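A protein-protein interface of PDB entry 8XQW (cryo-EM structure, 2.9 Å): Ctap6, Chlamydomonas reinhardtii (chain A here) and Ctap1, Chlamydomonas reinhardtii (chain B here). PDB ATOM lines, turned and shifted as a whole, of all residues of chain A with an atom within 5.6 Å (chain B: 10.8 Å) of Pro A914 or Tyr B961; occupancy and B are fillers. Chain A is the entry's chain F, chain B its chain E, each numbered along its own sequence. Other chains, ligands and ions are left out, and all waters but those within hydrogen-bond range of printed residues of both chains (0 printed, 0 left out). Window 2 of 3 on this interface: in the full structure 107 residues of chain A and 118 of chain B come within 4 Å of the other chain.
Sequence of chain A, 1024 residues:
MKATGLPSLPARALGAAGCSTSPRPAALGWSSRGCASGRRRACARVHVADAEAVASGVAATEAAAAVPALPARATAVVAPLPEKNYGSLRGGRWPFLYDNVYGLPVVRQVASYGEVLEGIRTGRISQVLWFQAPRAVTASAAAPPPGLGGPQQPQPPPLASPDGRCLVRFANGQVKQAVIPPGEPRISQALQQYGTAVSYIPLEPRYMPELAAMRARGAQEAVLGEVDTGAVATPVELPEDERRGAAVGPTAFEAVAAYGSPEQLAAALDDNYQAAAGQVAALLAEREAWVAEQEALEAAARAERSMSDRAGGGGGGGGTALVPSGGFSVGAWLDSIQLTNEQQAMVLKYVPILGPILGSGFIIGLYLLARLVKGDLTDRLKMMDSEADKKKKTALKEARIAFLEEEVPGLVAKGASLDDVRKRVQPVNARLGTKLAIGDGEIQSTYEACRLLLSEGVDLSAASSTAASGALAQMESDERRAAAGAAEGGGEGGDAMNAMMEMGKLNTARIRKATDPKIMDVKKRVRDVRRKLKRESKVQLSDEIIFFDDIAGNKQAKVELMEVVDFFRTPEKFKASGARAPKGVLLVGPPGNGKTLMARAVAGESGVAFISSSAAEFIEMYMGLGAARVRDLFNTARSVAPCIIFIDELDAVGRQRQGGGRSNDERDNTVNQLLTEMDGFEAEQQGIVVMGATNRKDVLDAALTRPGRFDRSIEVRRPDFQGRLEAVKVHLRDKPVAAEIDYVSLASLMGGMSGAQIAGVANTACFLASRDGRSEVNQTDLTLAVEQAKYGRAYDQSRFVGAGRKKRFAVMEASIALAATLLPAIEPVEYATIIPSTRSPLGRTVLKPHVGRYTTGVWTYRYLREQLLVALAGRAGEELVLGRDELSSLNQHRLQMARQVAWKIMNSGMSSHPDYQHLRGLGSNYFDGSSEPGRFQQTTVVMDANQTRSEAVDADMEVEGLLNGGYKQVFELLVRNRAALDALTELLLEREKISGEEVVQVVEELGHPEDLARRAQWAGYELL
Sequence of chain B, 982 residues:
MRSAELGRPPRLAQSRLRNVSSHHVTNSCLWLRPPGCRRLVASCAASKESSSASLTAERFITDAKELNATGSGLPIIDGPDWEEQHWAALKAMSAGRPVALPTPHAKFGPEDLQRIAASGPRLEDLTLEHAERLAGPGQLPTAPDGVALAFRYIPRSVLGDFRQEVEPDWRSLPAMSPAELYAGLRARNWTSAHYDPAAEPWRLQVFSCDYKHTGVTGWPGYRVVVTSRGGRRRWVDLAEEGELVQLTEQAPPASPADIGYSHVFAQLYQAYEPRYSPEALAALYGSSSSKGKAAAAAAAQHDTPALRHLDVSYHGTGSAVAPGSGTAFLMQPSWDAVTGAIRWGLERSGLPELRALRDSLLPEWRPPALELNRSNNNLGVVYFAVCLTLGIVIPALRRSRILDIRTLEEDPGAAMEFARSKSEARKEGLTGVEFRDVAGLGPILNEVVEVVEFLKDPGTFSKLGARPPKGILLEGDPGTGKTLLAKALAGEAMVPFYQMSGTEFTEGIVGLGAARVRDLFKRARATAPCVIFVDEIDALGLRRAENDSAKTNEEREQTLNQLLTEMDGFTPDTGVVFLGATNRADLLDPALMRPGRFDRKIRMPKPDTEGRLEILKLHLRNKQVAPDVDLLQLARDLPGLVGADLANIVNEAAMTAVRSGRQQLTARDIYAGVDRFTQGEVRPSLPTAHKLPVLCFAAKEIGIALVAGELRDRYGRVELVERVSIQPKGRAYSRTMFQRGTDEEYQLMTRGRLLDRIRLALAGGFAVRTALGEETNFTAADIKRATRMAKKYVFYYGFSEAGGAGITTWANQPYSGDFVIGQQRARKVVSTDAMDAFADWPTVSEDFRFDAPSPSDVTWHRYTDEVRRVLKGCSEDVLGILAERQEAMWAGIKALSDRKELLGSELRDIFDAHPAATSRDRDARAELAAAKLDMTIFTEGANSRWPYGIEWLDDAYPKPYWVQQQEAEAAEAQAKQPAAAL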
ATOM      1  N   SER A 912     -23.743  -7.822  -9.518  1.00  0.00           N
ATOM      2  CA  SER A 912     -23.064  -7.677  -8.245  1.00  0.00           C
ATOM      3  C   SER A 912     -21.893  -6.711  -8.305  1.00  0.00           C
ATOM      4  O   SER A 912     -21.225  -6.505  -7.290  1.00  0.00           O
ATOM      5  CB  SER A 912     -22.581  -9.032  -7.743  1.00  0.00           C
ATOM      6  OG  SER A 912     -21.470  -8.865  -6.892  1.00  0.00           O
ATOM      7  N   HIS A 913     -21.630  -6.129  -9.463  1.00  0.00           N
ATOM      8  CA  HIS A 913     -20.678  -5.040  -9.555  1.00  0.00           C
ATOM      9  C   HIS A 913     -21.167  -3.869  -8.708  1.00  0.00           C
ATOM     10  O   HIS A 913     -22.346  -3.514  -8.770  1.00  0.00           O
ATOM     11  CB  HIS A 913     -20.538  -4.620 -11.013  1.00  0.00           C
ATOM     12  CG  HIS A 913     -19.296  -3.850 -11.317  1.00  0.00           C
ATOM     13  ND1 HIS A 913     -18.642  -3.951 -12.522  1.00  0.00           N
ATOM     14  CD2 HIS A 913     -18.596  -2.957 -10.585  1.00  0.00           C
ATOM     15  CE1 HIS A 913     -17.589  -3.157 -12.517  1.00  0.00           C
ATOM     16  NE2 HIS A 913     -17.537  -2.545 -11.352  1.00  0.00           N
ATOM     17  N   PRO A 914     -20.307  -3.256  -7.897  1.00  0.00           N
ATOM     18  CA  PRO A 914     -20.770  -2.115  -7.100  1.00  0.00           C
ATOM     19  C   PRO A 914     -21.216  -0.925  -7.929  1.00  0.00           C
ATOM     20  O   PRO A 914     -22.161  -0.240  -7.530  1.00  0.00           O
ATOM     21  CB  PRO A 914     -19.551  -1.780  -6.231  1.00  0.00           C
ATOM     22  CG  PRO A 914     -18.415  -2.477  -6.867  1.00  0.00           C
ATOM     23  CD  PRO A 914     -18.984  -3.708  -7.459  1.00  0.00           C
ATOM     24  N   ASP A 915     -20.585  -0.657  -9.063  1.00  0.00           N
ATOM     25  CA  ASP A 915     -21.003   0.438  -9.924  1.00  0.00           C
ATOM     26  C   ASP A 915     -22.224   0.103 -10.743  1.00  0.00           C
ATOM     27  O   ASP A 915     -22.647   0.926 -11.555  1.00  0.00           O
ATOM     28  CB  ASP A 915     -19.879   0.835 -10.874  1.00  0.00           C
ATOM     29  CG  ASP A 915     -18.641   1.281 -10.149  1.00  0.00           C
ATOM     30  OD1 ASP A 915     -18.644   1.263  -8.904  1.00  0.00           O
ATOM     31  OD2 ASP A 915     -17.662   1.654 -10.824  1.00  0.00           O
ATOM     32  N   TYR A 916     -22.776  -1.089 -10.576  1.00  0.00           N
ATOM     33  CA  TYR A 916     -23.883  -1.547 -11.395  1.00  0.00           C
ATOM     34  C   TYR A 916     -25.030  -2.119 -10.604  1.00  0.00           C
ATOM     35  O   TYR A 916     -26.085  -2.342 -11.193  1.00  0.00           O
ATOM     36  CB  TYR A 916     -23.422  -2.636 -12.358  1.00  0.00           C
ATOM     37  CG  TYR A 916     -23.010  -2.175 -13.710  1.00  0.00           C
ATOM     38  CD1 TYR A 916     -23.944  -1.910 -14.674  1.00  0.00           C
ATOM     39  CD2 TYR A 916     -21.679  -2.045 -14.034  1.00  0.00           C
ATOM     40  CE1 TYR A 916     -23.569  -1.507 -15.911  1.00  0.00           C
ATOM     41  CE2 TYR A 916     -21.297  -1.644 -15.270  1.00  0.00           C
ATOM     42  CZ  TYR A 916     -22.249  -1.368 -16.207  1.00  0.00           C
ATOM     43  OH  TYR A 916     -21.882  -0.963 -17.462  1.00  0.00           O
ATOM     44  N   GLN A 917     -24.875  -2.382  -9.309  1.00  0.00           N
ATOM     45  CA  GLN A 917     -25.752  -3.342  -8.657  1.00  0.00           C
ATOM     46  C   GLN A 917     -27.202  -2.903  -8.718  1.00  0.00           C
ATOM     47  O   GLN A 917     -28.013  -3.525  -9.405  1.00  0.00           O
ATOM     48  CB  GLN A 917     -25.344  -3.567  -7.213  1.00  0.00           C
ATOM     49  CG  GLN A 917     -26.214  -4.602  -6.556  1.00  0.00           C
ATOM     50  CD  GLN A 917     -25.533  -5.293  -5.420  1.00  0.00           C
ATOM     51  OE1 GLN A 917     -25.945  -6.367  -5.000  1.00  0.00           O
ATOM     52  NE2 GLN A 917     -24.478  -4.686  -4.910  1.00  0.00           N
ATOM     53  N   LEU A 919     -28.148   0.287  -9.576  1.00  0.00           N
ATOM     54  CA  LEU A 919     -28.101   1.620 -10.156  1.00  0.00           C
ATOM     55  C   LEU A 919     -28.446   1.673 -11.629  1.00  0.00           C
ATOM     56  O   LEU A 919     -29.205   2.548 -12.037  1.00  0.00           O
ATOM     57  CB  LEU A 919     -26.718   2.228  -9.969  1.00  0.00           C
ATOM     58  CG  LEU A 919     -26.114   2.196  -8.581  1.00  0.00           C
ATOM     59  CD1 LEU A 919     -24.788   2.873  -8.633  1.00  0.00           C
ATOM     60  CD2 LEU A 919     -27.019   2.900  -7.628  1.00  0.00           C
ATOM     61  N   SER A 950     -13.610  -0.032 -19.321  1.00  0.00           N
ATOM     62  CA  SER A 950     -13.208  -1.138 -18.480  1.00  0.00           C
ATOM     63  C   SER A 950     -14.372  -1.671 -17.681  1.00  0.00           C
ATOM     64  O   SER A 950     -14.161  -2.448 -16.755  1.00  0.00           O
ATOM     65  CB  SER A 950     -12.089  -0.725 -17.533  1.00  0.00           C
ATOM     66  OG  SER A 950     -12.610  -0.498 -16.244  1.00  0.00           O
ATOM     67  N   ASP A 954     -15.730  -6.004 -17.508  1.00  0.00           N
ATOM     68  CA  ASP A 954     -16.428  -6.561 -16.354  1.00  0.00           C
ATOM     69  C   ASP A 954     -17.759  -7.170 -16.739  1.00  0.00           C
ATOM     70  O   ASP A 954     -18.139  -8.211 -16.204  1.00  0.00           O
ATOM     71  CB  ASP A 954     -16.630  -5.496 -15.303  1.00  0.00           C
ATOM     72  CG  ASP A 954     -15.350  -5.015 -14.765  1.00  0.00           C
ATOM     73  OD1 ASP A 954     -14.472  -4.744 -15.591  1.00  0.00           O
ATOM     74  OD2 ASP A 954     -15.212  -4.887 -13.538  1.00  0.00           O
ATOM     75  N   TRP B 946      -4.762 -11.851 -15.539  1.00  0.00           N
ATOM     76  CA  TRP B 946      -5.192 -10.544 -16.048  1.00  0.00           C
ATOM     77  C   TRP B 946      -4.400 -10.012 -17.229  1.00  0.00           C
ATOM     78  O   TRP B 946      -5.025  -9.674 -18.238  1.00  0.00           O
ATOM     79  CB  TRP B 946      -5.170  -9.464 -14.962  1.00  0.00           C
ATOM     80  CG  TRP B 946      -5.072  -8.068 -15.533  1.00  0.00           C
ATOM     81  CD1 TRP B 946      -4.094  -7.163 -15.292  1.00  0.00           C
ATOM     82  CD2 TRP B 946      -5.993  -7.427 -16.424  1.00  0.00           C
ATOM     83  NE1 TRP B 946      -4.336  -6.007 -15.975  1.00  0.00           N
ATOM     84  CE2 TRP B 946      -5.501  -6.144 -16.677  1.00  0.00           C
ATOM     85  CE3 TRP B 946      -7.180  -7.817 -17.035  1.00  0.00           C
ATOM     86  CZ2 TRP B 946      -6.147  -5.251 -17.509  1.00  0.00           C
ATOM     87  CZ3 TRP B 946      -7.822  -6.925 -17.859  1.00  0.00           C
ATOM     88  CH2 TRP B 946      -7.307  -5.661 -18.087  1.00  0.00           C
ATOM     89  N   TYR B 948      -2.800 -11.491 -19.418  1.00  0.00           N
ATOM     90  CA  TYR B 948      -2.920 -12.432 -20.529  1.00  0.00           C
ATOM     91  C   TYR B 948      -1.728 -12.339 -21.464  1.00  0.00           C
ATOM     92  O   TYR B 948      -1.863 -12.501 -22.673  1.00  0.00           O
ATOM     93  CB  TYR B 948      -4.220 -12.233 -21.308  1.00  0.00           C
ATOM     94  CG  TYR B 948      -5.453 -12.241 -20.449  1.00  0.00           C
ATOM     95  CD1 TYR B 948      -5.747 -13.313 -19.642  1.00  0.00           C
ATOM     96  CD2 TYR B 948      -6.322 -11.173 -20.445  1.00  0.00           C
ATOM     97  CE1 TYR B 948      -6.858 -13.318 -18.852  1.00  0.00           C
ATOM     98  CE2 TYR B 948      -7.434 -11.172 -19.655  1.00  0.00           C
ATOM     99  CZ  TYR B 948      -7.698 -12.248 -18.862  1.00  0.00           C
ATOM    100  OH  TYR B 948      -8.816 -12.256 -18.071  1.00  0.00           O
ATOM    101  N   TYR B 957      -5.544   0.099 -20.184  1.00  0.00           N
ATOM    102  CA  TYR B 957      -6.786  -0.205 -19.509  1.00  0.00           C
ATOM    103  C   TYR B 957      -6.620  -0.039 -18.010  1.00  0.00           C
ATOM    104  O   TYR B 957      -5.623  -0.512 -17.450  1.00  0.00           O
ATOM    105  CB  TYR B 957      -7.224  -1.631 -19.807  1.00  0.00           C
ATOM    106  CG  TYR B 957      -7.874  -1.799 -21.139  1.00  0.00           C
ATOM    107  CD1 TYR B 957      -7.133  -1.760 -22.294  1.00  0.00           C
ATOM    108  CD2 TYR B 957      -9.222  -1.991 -21.243  1.00  0.00           C
ATOM    109  CE1 TYR B 957      -7.719  -1.906 -23.509  1.00  0.00           C
ATOM    110  CE2 TYR B 957      -9.815  -2.141 -22.454  1.00  0.00           C
ATOM    111  CZ  TYR B 957      -9.061  -2.098 -23.583  1.00  0.00           C
ATOM    112  OH  TYR B 957      -9.662  -2.248 -24.801  1.00  0.00           O
ATOM    113  N   PRO B 958      -7.550   0.611 -17.324  1.00  0.00           N
ATOM    114  CA  PRO B 958      -7.589   0.487 -15.872  1.00  0.00           C
ATOM    115  C   PRO B 958      -7.912  -0.941 -15.508  1.00  0.00           C
ATOM    116  O   PRO B 958      -8.527  -1.671 -16.282  1.00  0.00           O
ATOM    117  CB  PRO B 958      -8.717   1.433 -15.463  1.00  0.00           C
ATOM    118  CG  PRO B 958      -8.913   2.311 -16.618  1.00  0.00           C
ATOM    119  CD  PRO B 958      -8.613   1.493 -17.810  1.00  0.00           C
ATOM    120  N   LYS B 959      -7.502  -1.342 -14.340  1.00  0.00           N
ATOM    121  CA  LYS B 959      -7.739  -2.724 -13.972  1.00  0.00           C
ATOM    122  C   LYS B 959      -9.207  -2.918 -13.618  1.00  0.00           C
ATOM    123  O   LYS B 959      -9.752  -2.143 -12.833  1.00  0.00           O
ATOM    124  CB  LYS B 959      -6.868  -3.128 -12.807  1.00  0.00           C
ATOM    125  CG  LYS B 959      -6.937  -4.588 -12.543  1.00  0.00           C
ATOM    126  CD  LYS B 959      -5.928  -5.009 -11.521  1.00  0.00           C
ATOM    127  CE  LYS B 959      -4.541  -4.707 -11.986  1.00  0.00           C
ATOM    128  NZ  LYS B 959      -3.564  -5.407 -11.129  1.00  0.00           N
ATOM    129  N   PRO B 960      -9.874  -3.916 -14.185  1.00  0.00           N
ATOM    130  CA  PRO B 960     -11.287  -4.138 -13.883  1.00  0.00           C
ATOM    131  C   PRO B 960     -11.510  -4.467 -12.419  1.00  0.00           C
ATOM    132  O   PRO B 960     -10.590  -4.505 -11.607  1.00  0.00           O
ATOM    133  CB  PRO B 960     -11.644  -5.322 -14.773  1.00  0.00           C
ATOM    134  CG  PRO B 960     -10.719  -5.229 -15.884  1.00  0.00           C
ATOM    135  CD  PRO B 960      -9.435  -4.733 -15.319  1.00  0.00           C
ATOM    136  N   TYR B 961     -12.772  -4.692 -12.081  1.00  0.00           N
ATOM    137  CA  TYR B 961     -13.105  -4.981 -10.694  1.00  0.00           C
ATOM    138  C   TYR B 961     -12.954  -6.461 -10.384  1.00  0.00           C
ATOM    139  O   TYR B 961     -12.365  -6.831  -9.361  1.00  0.00           O
ATOM    140  CB  TYR B 961     -14.519  -4.506 -10.403  1.00  0.00           C
ATOM    141  CG  TYR B 961     -15.063  -4.939  -9.074  1.00  0.00           C
ATOM    142  CD1 TYR B 961     -14.585  -4.402  -7.901  1.00  0.00           C
ATOM    143  CD2 TYR B 961     -16.074  -5.870  -8.996  1.00  0.00           C
ATOM    144  CE1 TYR B 961     -15.090  -4.790  -6.694  1.00  0.00           C
ATOM    145  CE2 TYR B 961     -16.581  -6.261  -7.798  1.00  0.00           C
ATOM    146  CZ  TYR B 961     -16.087  -5.723  -6.650  1.00  0.00           C
ATOM    147  OH  TYR B 961     -16.605  -6.125  -5.445  1.00  0.00           O
ATOM    148  N   TRP B 962     -13.463  -7.317 -11.260  1.00  0.00           N
ATOM    149  CA  TRP B 962     -13.364  -8.746 -11.015  1.00  0.00           C
ATOM    150  C   TRP B 962     -11.926  -9.219 -11.068  1.00  0.00           C
ATOM    151  O   TRP B 962     -11.566 -10.182 -10.388  1.00  0.00           O
ATOM    152  CB  TRP B 962     -14.221  -9.498 -12.017  1.00  0.00           C
ATOM    153  CG  TRP B 962     -15.641  -9.122 -11.928  1.00  0.00           C
ATOM    154  CD1 TRP B 962     -16.365  -8.465 -12.858  1.00  0.00           C
ATOM    155  CD2 TRP B 962     -16.516  -9.366 -10.832  1.00  0.00           C
ATOM    156  NE1 TRP B 962     -17.647  -8.288 -12.420  1.00  0.00           N
ATOM    157  CE2 TRP B 962     -17.763  -8.831 -11.171  1.00  0.00           C
ATOM    158  CE3 TRP B 962     -16.369  -9.992  -9.597  1.00  0.00           C
ATOM    159  CZ2 TRP B 962     -18.854  -8.903 -10.327  1.00  0.00           C
ATOM    160  CZ3 TRP B 962     -17.453 -10.060  -8.759  1.00  0.00           C
ATOM    161  CH2 TRP B 962     -18.679  -9.520  -9.126  1.00  0.00           C
ATOM    162  N   VAL B 963     -11.081  -8.546 -11.842  1.00  0.00           N
ATOM    163  CA  VAL B 963      -9.668  -8.896 -11.857  1.00  0.00           C
ATOM    164  C   VAL B 963      -9.035  -8.592 -10.510  1.00  0.00           C
ATOM    165  O   VAL B 963      -8.225  -9.371  -9.998  1.00  0.00           O
ATOM    166  CB  VAL B 963      -8.956  -8.158 -12.996  1.00  0.00           C
ATOM    167  CG1 VAL B 963      -7.490  -8.090 -12.724  1.00  0.00           C
ATOM    168  CG2 VAL B 963      -9.215  -8.851 -14.300  1.00  0.00           C
ATOM    169  N   GLN B 964      -9.391  -7.458  -9.911  1.00  0.00           N
ATOM    170  CA  GLN B 964      -8.900  -7.157  -8.574  1.00  0.00           C
ATOM    171  C   GLN B 964      -9.387  -8.187  -7.573  1.00  0.00           C
ATOM    172  O   GLN B 964      -8.640  -8.600  -6.681  1.00  0.00           O
ATOM    173  CB  GLN B 964      -9.345  -5.767  -8.148  1.00  0.00           C
ATOM    174  CG  GLN B 964      -8.824  -4.653  -9.005  1.00  0.00           C
ATOM    175  CD  GLN B 964      -9.538  -3.357  -8.728  1.00  0.00           C
ATOM    176  OE1 GLN B 964      -9.480  -2.418  -9.516  1.00  0.00           O
ATOM    177  NE2 GLN B 964     -10.229  -3.298  -7.600  1.00  0.00           N
ATOM    178  N   GLN B 965     -10.638  -8.624  -7.709  1.00  0.00           N
ATOM    179  CA  GLN B 965     -11.161  -9.641  -6.802  1.00  0.00           C
ATOM    180  C   GLN B 965     -10.399 -10.951  -6.942  1.00  0.00           C
ATOM    181  O   GLN B 965     -10.081 -11.608  -5.944  1.00  0.00           O
ATOM    182  CB  GLN B 965     -12.642  -9.857  -7.070  1.00  0.00           C
ATOM    183  CG  GLN B 965     -13.473  -8.684  -6.680  1.00  0.00           C
ATOM    184  CD  GLN B 965     -13.152  -8.227  -5.291  1.00  0.00           C
ATOM    185  OE1 GLN B 965     -13.350  -8.961  -4.329  1.00  0.00           O
ATOM    186  NE2 GLN B 965     -12.646  -7.011  -5.169  1.00  0.00           N
ATOM    187  N   GLN B 966     -10.121 -11.363  -8.179  1.00  0.00           N
ATOM    188  CA  GLN B 966      -9.358 -12.585  -8.394  1.00  0.00           C
ATOM    189  C   GLN B 966      -7.962 -12.469  -7.811  1.00  0.00           C
ATOM    190  O   GLN B 966      -7.468 -13.408  -7.178  1.00  0.00           O
ATOM    191  CB  GLN B 966      -9.276 -12.905  -9.879  1.00  0.00           C
ATOM    192  CG  GLN B 966     -10.483 -13.610 -10.416  1.00  0.00           C
ATOM    193  CD  GLN B 966     -10.425 -13.756 -11.911  1.00  0.00           C
ATOM    194  OE1 GLN B 966      -9.415 -13.441 -12.535  1.00  0.00           O
ATOM    195  NE2 GLN B 966     -11.515 -14.224 -12.501  1.00  0.00           N
ATOM    196  N   GLU B 967      -7.298 -11.338  -8.033  1.00  0.00           N
ATOM    197  CA  GLU B 967      -5.991 -11.137  -7.425  1.00  0.00           C
ATOM    198  C   GLU B 967      -6.074 -11.244  -5.913  1.00  0.00           C
ATOM    199  O   GLU B 967      -5.207 -11.855  -5.283  1.00  0.00           O
ATOM    200  CB  GLU B 967      -5.419  -9.786  -7.831  1.00  0.00           C
ATOM    201  CG  GLU B 967      -4.994  -9.694  -9.278  1.00  0.00           C
ATOM    202  CD  GLU B 967      -4.502  -8.309  -9.642  1.00  0.00           C
ATOM    203  OE1 GLU B 967      -4.333  -7.479  -8.727  1.00  0.00           O
ATOM    204  OE2 GLU B 967      -4.292  -8.043 -10.843  1.00  0.00           O
ATOM    205  N   ALA B 968      -7.122 -10.680  -5.315  1.00  0.00           N
ATOM    206  CA  ALA B 968      -7.250 -10.704  -3.861  1.00  0.00           C
ATOM    207  C   ALA B 968      -7.417 -12.124  -3.346  1.00  0.00           C
ATOM    208  O   ALA B 968      -6.744 -12.536  -2.393  1.00  0.00           O
ATOM    209  CB  ALA B 968      -8.426  -9.835  -3.426  1.00  0.00           C
ATOM    210  N   GLU B 969      -8.324 -12.889  -3.953  1.00  0.00           N
ATOM    211  CA  GLU B 969      -8.556 -14.245  -3.468  1.00  0.00           C
ATOM    212  C   GLU B 969      -7.346 -15.137  -3.717  1.00  0.00           C
ATOM    213  O   GLU B 969      -7.007 -15.976  -2.876  1.00  0.00           O
ATOM    214  CB  GLU B 969      -9.816 -14.840  -4.096  1.00  0.00           C
ATOM    215  CG  GLU B 969      -9.903 -14.737  -5.601  1.00  0.00           C
ATOM    216  CD  GLU B 969      -9.343 -15.951  -6.315  1.00  0.00           C
ATOM    217  OE1 GLU B 969      -9.440 -16.002  -7.559  1.00  0.00           O
ATOM    218  OE2 GLU B 969      -8.803 -16.850  -5.639  1.00  0.00           O
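N of Tyr B961 sits at hydrogen-bond distance from OD2 of Asp A954 (2.8 Å).
Of the 9 printed residues of chain A, 5 touch a printed residue of chain B.
Hydrophobic or aromatic side chains of chain A that line the printed part of chain B: His A913 and Pro A914.
Among the printed residues, no Asp or Glu carboxylate lies within 4 Å of a Lys or Arg side-chain nitrogen of the other chain.
Among the printed residues, pairs that only touch across the chains: Ser A912 with Trp B962 (3.6 Å), His A913 with Tyr B961 (3.7 Å), Pro A914 with Tyr B961 (3.5 Å), Ser A950 with Pro B958 (3.9 Å), Asp A954 with Pro B960 (3.0 Å) and Asp A954 with Trp B962 (3.8 Å).
Ser A912 touches just one residue of chain B: Trp B962.
Pro A914 touches one residue of chain B.
No residue of chain B comes within 4 Å of Asp A915.
Of the printed residues of chain A, Pro B958 touches Ser A950 (3.9 Å).
Printed residues of chain A within 4 Å of Pro B960: Asp A954 (3.0 Å).
Of chain A, only His A913, Pro A914 and Asp A954 come within 4 Å of Tyr B961.
Of the printed residues of chain A, Trp B962 touches Ser A912 (3.6 Å) and Asp A954 (3.8 Å).
The nearest residue of chain B that does not touch Pro A914 is Trp B962 (5.9 Å).
The nearest residue of chain A that does not touch Tyr B961 is Ser A912 (4.7 Å).
The backbone carbonyl oxygen (O) of Pro B960 lies close to the side-chain amide oxygen (OE1) of Gln B964, at 3.2 Å.
The side-chain carboxylate (OD1) of Asp A954 sits close to the backbone carbonyl oxygen (O) of Ser A950, at 2.6 Å.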
